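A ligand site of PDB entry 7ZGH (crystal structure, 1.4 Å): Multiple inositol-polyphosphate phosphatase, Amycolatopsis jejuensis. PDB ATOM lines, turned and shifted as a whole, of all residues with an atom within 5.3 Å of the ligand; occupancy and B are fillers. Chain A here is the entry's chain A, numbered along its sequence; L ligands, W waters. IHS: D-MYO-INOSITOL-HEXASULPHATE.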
ATOM      1  N   SER A  11      -8.192   7.061  29.175  1.00  0.00           N
ATOM      2  CA  SER A  11      -6.827   6.922  29.657  1.00  0.00           C
ATOM      3  C   SER A  11      -6.046   8.237  29.656  1.00  0.00           C
ATOM      4  O   SER A  11      -4.903   8.263  30.127  1.00  0.00           O
ATOM      5  CB  SER A  11      -6.096   5.882  28.798  1.00  0.00           C
ATOM      6  OG  SER A  11      -6.032   6.300  27.433  1.00  0.00           O
ATOM      7  N   LYS A  12      -6.632   9.310  29.150  1.00  0.00           N
ATOM      8  CA  LYS A  12      -6.021  10.633  29.209  1.00  0.00           C
ATOM      9  C   LYS A  12      -6.560  11.478  30.359  1.00  0.00           C
ATOM     10  O   LYS A  12      -6.167  12.640  30.502  1.00  0.00           O
ATOM     11  CB  LYS A  12      -6.135  11.373  27.852  1.00  0.00           C
ATOM     12  CG  LYS A  12      -5.240  10.785  26.737  1.00  0.00           C
ATOM     13  CD  LYS A  12      -5.682   9.443  26.204  1.00  0.00           C
ATOM     14  CE  LYS A  12      -4.791   9.038  25.045  1.00  0.00           C
ATOM     15  NZ  LYS A  12      -5.369   7.850  24.404  1.00  0.00           N
ATOM     16  N   ARG A  41       2.091   5.152  36.952  1.00  0.00           N
ATOM     17  CA  ARG A  41       2.231   5.685  35.614  1.00  0.00           C
ATOM     18  C   ARG A  41       2.798   7.100  35.679  1.00  0.00           C
ATOM     19  O   ARG A  41       2.718   7.791  36.700  1.00  0.00           O
ATOM     20  CB  ARG A  41       0.851   5.772  34.958  1.00  0.00           C
ATOM     21  CG  ARG A  41       0.854   6.180  33.486  1.00  0.00           C
ATOM     22  CD  ARG A  41      -0.563   6.223  32.960  1.00  0.00           C
ATOM     23  NE  ARG A  41      -0.633   6.602  31.558  1.00  0.00           N
ATOM     24  CZ  ARG A  41      -1.768   6.893  30.943  1.00  0.00           C
ATOM     25  NH1 ARG A  41      -2.925   6.888  31.580  1.00  0.00           N
ATOM     26  NH2 ARG A  41      -1.738   7.240  29.650  1.00  0.00           N
ATOM     27  N   HIS A  42       3.384   7.534  34.577  1.00  0.00           N
ATOM     28  CA  HIS A  42       3.757   8.930  34.450  1.00  0.00           C
ATOM     29  C   HIS A  42       2.528   9.812  34.651  1.00  0.00           C
ATOM     30  O   HIS A  42       1.390   9.390  34.485  1.00  0.00           O
ATOM     31  CB  HIS A  42       4.333   9.197  33.055  1.00  0.00           C
ATOM     32  CG  HIS A  42       3.412   8.815  31.932  1.00  0.00           C
ATOM     33  ND1 HIS A  42       2.318   9.563  31.574  1.00  0.00           N
ATOM     34  CD2 HIS A  42       3.424   7.738  31.109  1.00  0.00           C
ATOM     35  CE1 HIS A  42       1.700   8.986  30.560  1.00  0.00           C
ATOM     36  NE2 HIS A  42       2.347   7.866  30.252  1.00  0.00           N
ATOM     37  N   ARG A  45       0.408  14.403  30.375  1.00  0.00           N
ATOM     38  CA  ARG A  45       1.407  14.597  29.329  1.00  0.00           C
ATOM     39  C   ARG A  45       0.735  15.197  28.099  1.00  0.00           C
ATOM     40  O   ARG A  45      -0.490  15.241  27.984  1.00  0.00           O
ATOM     41  CB  ARG A  45       2.063  13.270  28.928  1.00  0.00           C
ATOM     42  CG  ARG A  45       1.095  12.169  28.469  1.00  0.00           C
ATOM     43  CD  ARG A  45       1.815  11.108  27.630  1.00  0.00           C
ATOM     44  NE  ARG A  45       0.975   9.976  27.219  1.00  0.00           N
ATOM     45  CZ  ARG A  45       0.136   9.986  26.183  1.00  0.00           C
ATOM     46  NH1 ARG A  45      -0.041  11.084  25.452  1.00  0.00           N
ATOM     47  NH2 ARG A  45      -0.536   8.879  25.884  1.00  0.00           N
ATOM     48  N   THR A  48       1.141  12.138  21.983  1.00  0.00           N
ATOM     49  CA  THR A  48       2.353  11.543  21.449  1.00  0.00           C
ATOM     50  C   THR A  48       2.585  11.895  19.992  1.00  0.00           C
ATOM     51  O   THR A  48       3.716  11.765  19.517  1.00  0.00           O
ATOM     52  CB  THR A  48       2.294  10.018  21.554  1.00  0.00           C
ATOM     53  OG1 THR A  48       1.058   9.559  21.014  1.00  0.00           O
ATOM     54  CG2 THR A  48       2.436   9.602  22.998  1.00  0.00           C
ATOM     55  N   LYS A  49       1.541  12.315  19.278  1.00  0.00           N
ATOM     56  CA  LYS A  49       1.608  12.586  17.858  1.00  0.00           C
ATOM     57  C   LYS A  49       0.864  13.880  17.565  1.00  0.00           C
ATOM     58  O   LYS A  49      -0.142  14.196  18.203  1.00  0.00           O
ATOM     59  CB  LYS A  49       0.959  11.460  17.048  1.00  0.00           C
ATOM     60  CG  LYS A  49       1.589  10.105  17.298  1.00  0.00           C
ATOM     61  CD  LYS A  49       0.925   9.063  16.419  1.00  0.00           C
ATOM     62  CE  LYS A  49       1.863   7.902  16.154  1.00  0.00           C
ATOM     63  NZ  LYS A  49       2.744   7.673  17.328  1.00  0.00           N
ATOM     64  N   ARG A 138       9.376  10.732  29.710  1.00  0.00           N
ATOM     65  CA  ARG A 138       8.305  11.089  30.648  1.00  0.00           C
ATOM     66  C   ARG A 138       8.336  10.238  31.907  1.00  0.00           C
ATOM     67  O   ARG A 138       7.943  10.706  32.979  1.00  0.00           O
ATOM     68  CB  ARG A 138       6.913  11.058  29.965  1.00  0.00           C
ATOM     69  CG  ARG A 138       6.450   9.731  29.359  1.00  0.00           C
ATOM     70  CD  ARG A 138       5.022   9.877  28.800  1.00  0.00           C
ATOM     71  NE  ARG A 138       4.582   8.717  28.025  1.00  0.00           N
ATOM     72  CZ  ARG A 138       4.825   8.529  26.727  1.00  0.00           C
ATOM     73  NH1 ARG A 138       5.502   9.411  26.008  1.00  0.00           N
ATOM     74  NH2 ARG A 138       4.375   7.421  26.146  1.00  0.00           N
ATOM     75  N   TYR A 172       8.289  -2.677  31.882  1.00  0.00           N
ATOM     76  CA  TYR A 172       8.106  -2.411  30.457  1.00  0.00           C
ATOM     77  C   TYR A 172       7.821  -3.714  29.736  1.00  0.00           C
ATOM     78  O   TYR A 172       8.179  -3.915  28.564  1.00  0.00           O
ATOM     79  CB  TYR A 172       9.327  -1.661  29.904  1.00  0.00           C
ATOM     80  CG  TYR A 172       9.078  -0.720  28.740  1.00  0.00           C
ATOM     81  CD1 TYR A 172       7.863  -0.064  28.586  1.00  0.00           C
ATOM     82  CD2 TYR A 172      10.090  -0.442  27.820  1.00  0.00           C
ATOM     83  CE1 TYR A 172       7.656   0.820  27.523  1.00  0.00           C
ATOM     84  CE2 TYR A 172       9.890   0.441  26.765  1.00  0.00           C
ATOM     85  CZ  TYR A 172       8.672   1.067  26.623  1.00  0.00           C
ATOM     86  OH  TYR A 172       8.485   1.939  25.569  1.00  0.00           O
ATOM     87  N   HIS A 174       5.352  -5.240  28.361  1.00  0.00           N
ATOM     88  CA  HIS A 174       4.650  -5.358  27.086  1.00  0.00           C
ATOM     89  C   HIS A 174       5.596  -5.204  25.897  1.00  0.00           C
ATOM     90  O   HIS A 174       5.222  -5.601  24.782  1.00  0.00           O
ATOM     91  CB  HIS A 174       3.434  -4.433  26.984  1.00  0.00           C
ATOM     92  CG  HIS A 174       3.751  -3.005  26.660  1.00  0.00           C
ATOM     93  ND1 HIS A 174       4.248  -2.126  27.594  1.00  0.00           N
ATOM     94  CD2 HIS A 174       3.612  -2.302  25.513  1.00  0.00           C
ATOM     95  CE1 HIS A 174       4.402  -0.936  27.030  1.00  0.00           C
ATOM     96  NE2 HIS A 174       4.022  -1.016  25.770  1.00  0.00           N
ATOM     97  N   LYS A 175       6.800  -4.679  26.110  1.00  0.00           N
ATOM     98  CA  LYS A 175       7.751  -4.509  25.023  1.00  0.00           C
ATOM     99  C   LYS A 175       8.942  -5.460  25.077  1.00  0.00           C
ATOM    100  O   LYS A 175       9.767  -5.431  24.156  1.00  0.00           O
ATOM    101  CB  LYS A 175       8.267  -3.066  24.991  1.00  0.00           C
ATOM    102  CG  LYS A 175       7.164  -2.045  25.026  1.00  0.00           C
ATOM    103  CD  LYS A 175       6.706  -1.692  23.639  1.00  0.00           C
ATOM    104  CE  LYS A 175       7.356  -0.418  23.159  1.00  0.00           C
ATOM    105  NZ  LYS A 175       7.455  -0.397  21.676  1.00  0.00           N
ATOM    106  N   LYS A 278      -7.739  -5.016  24.340  1.00  0.00           N
ATOM    107  CA  LYS A 278      -6.330  -4.950  23.994  1.00  0.00           C
ATOM    108  C   LYS A 278      -5.444  -5.022  25.218  1.00  0.00           C
ATOM    109  O   LYS A 278      -4.385  -5.649  25.179  1.00  0.00           O
ATOM    110  CB  LYS A 278      -6.033  -3.669  23.207  1.00  0.00           C
ATOM    111  CG  LYS A 278      -4.602  -3.540  22.760  1.00  0.00           C
ATOM    112  CD  LYS A 278      -4.387  -2.282  21.935  1.00  0.00           C
ATOM    113  CE  LYS A 278      -2.979  -2.197  21.398  1.00  0.00           C
ATOM    114  NZ  LYS A 278      -2.750  -0.905  20.668  1.00  0.00           N
ATOM    115  N   LYS A 279      -5.870  -4.372  26.322  1.00  0.00           N
ATOM    116  CA  LYS A 279      -5.010  -4.189  27.488  1.00  0.00           C
ATOM    117  C   LYS A 279      -5.609  -4.721  28.784  1.00  0.00           C
ATOM    118  O   LYS A 279      -4.859  -5.091  29.690  1.00  0.00           O
ATOM    119  CB  LYS A 279      -4.685  -2.703  27.665  1.00  0.00           C
ATOM    120  CG  LYS A 279      -4.219  -2.022  26.375  1.00  0.00           C
ATOM    121  CD  LYS A 279      -4.019  -0.550  26.588  1.00  0.00           C
ATOM    122  CE  LYS A 279      -3.372   0.066  25.364  1.00  0.00           C
ATOM    123  NZ  LYS A 279      -3.132   1.515  25.581  1.00  0.00           N
ATOM    124  N   HIS A 320       4.263   2.786  32.531  1.00  0.00           N
ATOM    125  CA  HIS A 320       3.235   3.195  31.583  1.00  0.00           C
ATOM    126  C   HIS A 320       1.889   2.583  31.929  1.00  0.00           C
ATOM    127  O   HIS A 320       1.782   1.650  32.749  1.00  0.00           O
ATOM    128  CB  HIS A 320       3.634   2.783  30.151  1.00  0.00           C
ATOM    129  CG  HIS A 320       4.909   3.396  29.670  1.00  0.00           C
ATOM    130  ND1 HIS A 320       4.926   4.524  28.876  1.00  0.00           N
ATOM    131  CD2 HIS A 320       6.206   3.034  29.837  1.00  0.00           C
ATOM    132  CE1 HIS A 320       6.181   4.828  28.587  1.00  0.00           C
ATOM    133  NE2 HIS A 320       6.973   3.949  29.164  1.00  0.00           N
ATOM    134  N   ALA A 321       0.845   3.081  31.260  1.00  0.00           N
ATOM    135  CA  ALA A 321      -0.495   2.545  31.466  1.00  0.00           C
ATOM    136  C   ALA A 321      -0.554   1.060  31.125  1.00  0.00           C
ATOM    137  O   ALA A 321      -1.279   0.295  31.766  1.00  0.00           O
ATOM    138  CB  ALA A 321      -1.516   3.301  30.611  1.00  0.00           C
ATOM    139  N   GLU A 322       0.200   0.637  30.101  1.00  0.00           N
ATOM    140  CA  GLU A 322       0.151  -0.754  29.658  1.00  0.00           C
ATOM    141  C   GLU A 322       0.773  -1.721  30.648  1.00  0.00           C
ATOM    142  O   GLU A 322       0.652  -2.939  30.460  1.00  0.00           O
ATOM    143  CB  GLU A 322       0.805  -0.894  28.278  1.00  0.00           C
ATOM    144  CG  GLU A 322       0.890  -2.330  27.748  1.00  0.00           C
ATOM    145  CD  GLU A 322      -0.393  -3.157  27.892  1.00  0.00           C
ATOM    146  OE1 GLU A 322      -1.500  -2.591  28.016  1.00  0.00           O
ATOM    147  OE2 GLU A 322      -0.290  -4.397  27.870  1.00  0.00           O
ATOM    148  N   GLU A 323       1.431  -1.239  31.697  1.00  0.00           N
ATOM    149  CA  GLU A 323       1.826  -2.087  32.817  1.00  0.00           C
ATOM    150  C   GLU A 323       0.826  -2.045  33.964  1.00  0.00           C
ATOM    151  O   GLU A 323       0.537  -3.096  34.548  1.00  0.00           O
ATOM    152  CB  GLU A 323       3.249  -1.718  33.289  1.00  0.00           C
ATOM    153  CG  GLU A 323       4.387  -2.271  32.393  1.00  0.00           C
ATOM    154  CD  GLU A 323       4.393  -1.765  30.954  1.00  0.00           C
ATOM    155  OE1 GLU A 323       4.231  -0.550  30.713  1.00  0.00           O
ATOM    156  OE2 GLU A 323       4.573  -2.608  30.044  1.00  0.00           O
ATOM    157  N   MET A 361      -4.155   9.303  34.033  1.00  0.00           N
ATOM    158  CA  MET A 361      -2.773   9.739  34.183  1.00  0.00           C
ATOM    159  C   MET A 361      -2.368   9.547  35.642  1.00  0.00           C
ATOM    160  O   MET A 361      -3.198   9.629  36.553  1.00  0.00           O
ATOM    161  CB  MET A 361      -2.579  11.181  33.754  1.00  0.00           C
ATOM    162  CG  MET A 361      -2.879  11.307  32.268  1.00  0.00           C
ATOM    163  SD  MET A 361      -1.463  10.749  31.301  1.00  0.00           S
ATOM    164  CE  MET A 361      -2.248  10.571  29.688  1.00  0.00           C
HETATM  165  C1  IHS L   1       1.689   4.077  24.898  1.00  0.00           C
HETATM  166  O1  IHS L   1       3.069   4.106  25.424  1.00  0.00           O
HETATM  167  S1  IHS L   1       3.770   2.750  25.809  1.00  0.00           S
HETATM  168  C2  IHS L   1       1.786   4.379  23.418  1.00  0.00           C
HETATM  169  O2  IHS L   1       3.723   1.924  24.620  1.00  0.00           O
HETATM  170  S2  IHS L   1       3.909   5.796  22.575  1.00  0.00           S
HETATM  171  C3  IHS L   1       0.400   4.584  22.830  1.00  0.00           C
HETATM  172  O3  IHS L   1       5.107   3.108  26.207  1.00  0.00           O
HETATM  173  S3  IHS L   1       0.433   3.953  20.319  1.00  0.00           S
HETATM  174  C4  IHS L   1      -0.352   5.661  23.581  1.00  0.00           C
HETATM  175  O4  IHS L   1       2.947   2.243  26.876  1.00  0.00           O
HETATM  176  S4  IHS L   1      -2.145   7.211  22.446  1.00  0.00           S
HETATM  177  C5  IHS L   1      -0.504   5.215  25.014  1.00  0.00           C
HETATM  178  S5  IHS L   1      -2.671   5.752  26.404  1.00  0.00           S
HETATM  179  C6  IHS L   1       0.891   5.159  25.609  1.00  0.00           C
HETATM  180  S6  IHS L   1       1.348   5.830  28.103  1.00  0.00           S
HETATM  181  O12 IHS L   1       2.509   5.670  23.346  1.00  0.00           O
HETATM  182  O13 IHS L   1       0.540   5.020  21.431  1.00  0.00           O
HETATM  183  O14 IHS L   1      -1.697   5.805  22.967  1.00  0.00           O
HETATM  184  O15 IHS L   1      -1.318   6.206  25.755  1.00  0.00           O
HETATM  185  O16 IHS L   1       0.792   4.830  27.037  1.00  0.00           O
HETATM  186  O22 IHS L   1       4.413   4.449  22.385  1.00  0.00           O
HETATM  187  O23 IHS L   1       1.332   2.918  20.652  1.00  0.00           O
HETATM  188  O24 IHS L   1      -3.504   7.064  22.061  1.00  0.00           O
HETATM  189  O25 IHS L   1      -3.542   5.302  25.376  1.00  0.00           O
HETATM  190  O26 IHS L   1       0.938   5.249  29.332  1.00  0.00           O
HETATM  191  O32 IHS L   1       3.585   6.455  21.327  1.00  0.00           O
HETATM  192  O33 IHS L   1      -1.000   3.388  20.429  1.00  0.00           O
HETATM  193  O34 IHS L   1      -1.842   8.202  23.406  1.00  0.00           O
HETATM  194  O35 IHS L   1      -3.120   6.870  27.147  1.00  0.00           O
HETATM  195  O36 IHS L   1       2.734   5.953  27.871  1.00  0.00           O
HETATM  196  O42 IHS L   1       4.759   6.597  23.422  1.00  0.00           O
HETATM  197  O43 IHS L   1       0.558   4.633  19.084  1.00  0.00           O
HETATM  198  O44 IHS L   1      -1.295   7.405  21.185  1.00  0.00           O
HETATM  199  O45 IHS L   1      -2.343   4.594  27.356  1.00  0.00           O
HETATM  200  O46 IHS L   1       0.637   7.160  27.865  1.00  0.00           O
HETATM  201  O   HOH W   1      -5.293   2.850  26.825  1.00  0.00           O
HETATM  202  O   HOH W   2      -1.444  10.802  23.001  1.00  0.00           O
HETATM  203  O   HOH W   3       2.914  -0.139  23.024  1.00  0.00           O
HETATM  204  O   HOH W   4       6.021   9.256  23.175  1.00  0.00           O
HETATM  205  O   HOH W   5      -4.589   4.238  23.089  1.00  0.00           O
HETATM  206  O   HOH W   6       1.460   7.203  19.984  1.00  0.00           O
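Tyr 172 touches the ligand (OH to O3, 3.6 Å).
Hydrophobic or aromatic side chains that line the ligand: His 42, Tyr 172, His 174, His 320 and Ala 321.
12 residues have an atom within 4 Å of the ligand: Ser 11, Lys 12, Arg 41, His 42, Arg 45, Thr 48, Arg 138, Tyr 172, His 174, Lys 279, His 320 and Ala 321.
Water W6 lies within hydrogen-bond range of OG1 of Thr 48, O32 of the ligand and NZ of Lys 49.
Water W2 lies within hydrogen-bond range of O34 of the ligand, NH1 of Arg 45 and N of Thr 48.
Water W3 lies within hydrogen-bond range of an oxygen (O2) of the ligand and a ring nitrogen (NE2) of His 174.
Water W4 lies within hydrogen-bond range of the guanidinium group (NH1) of Arg 138 (2.9 Å) and an oxygen (O42) of the ligand (3.0 Å).
Water W1 bridges NZ of Lys 279 (2.8 Å) and O25 of the ligand (3.3 Å).
A ring nitrogen (NE2) of His 42 lies within hydrogen-bond range of the guanidinium group (NE) of Arg 138.
The backbone carbonyl oxygen (O) of Ser 11 sits at hydrogen-bond distance from the guanidinium group (NH1) of Arg 41.
The guanidinium group (NE) of Arg 41 lies close to a ring nitrogen (NE2) of His 42 (3.5 Å).
NZ of Lys 12 sits close to OG of Ser 11 (3.5 Å).
The side-chain carboxylate of Glu 323 is in hydrogen-bond range of a ring nitrogen (ND1) of His 174 (2.5 Å).
O46 of the ligand is in salt-bridge range of NH2 of Arg 45 (2.9 Å).
An oxygen (O36) of the ligand is in salt-bridge range of the guanidinium group of Arg 138 (2.8 Å).
A ring nitrogen (ND1) of His 320 lies within hydrogen-bond range of an oxygen (O36) of the ligand (2.8 Å).
The guanidinium group of Arg 41 lies within salt-bridge range of an oxygen (O35) of the ligand, at 2.9 Å.
N of Ala 321 is in hydrogen-bond range of O26 of the ligand.
OG of Ser 11 sits at hydrogen-bond distance from O35 of the ligand (3.0 Å).
NE2 of His 42 lies within hydrogen-bond range of O46 of the ligand, at 3.0 Å.
NZ of Lys 12 is in salt-bridge range of O24 of the ligand (3.1 Å).
A ring nitrogen (NE2) of His 174 sits at hydrogen-bond distance from an oxygen (O2) of the ligand.
OG1 of Thr 48 sits at hydrogen-bond distance from O44 of the ligand (3.2 Å).
The side-chain amino group of Lys 279 lies within salt-bridge range of an oxygen (O45) of the ligand (3.6 Å).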
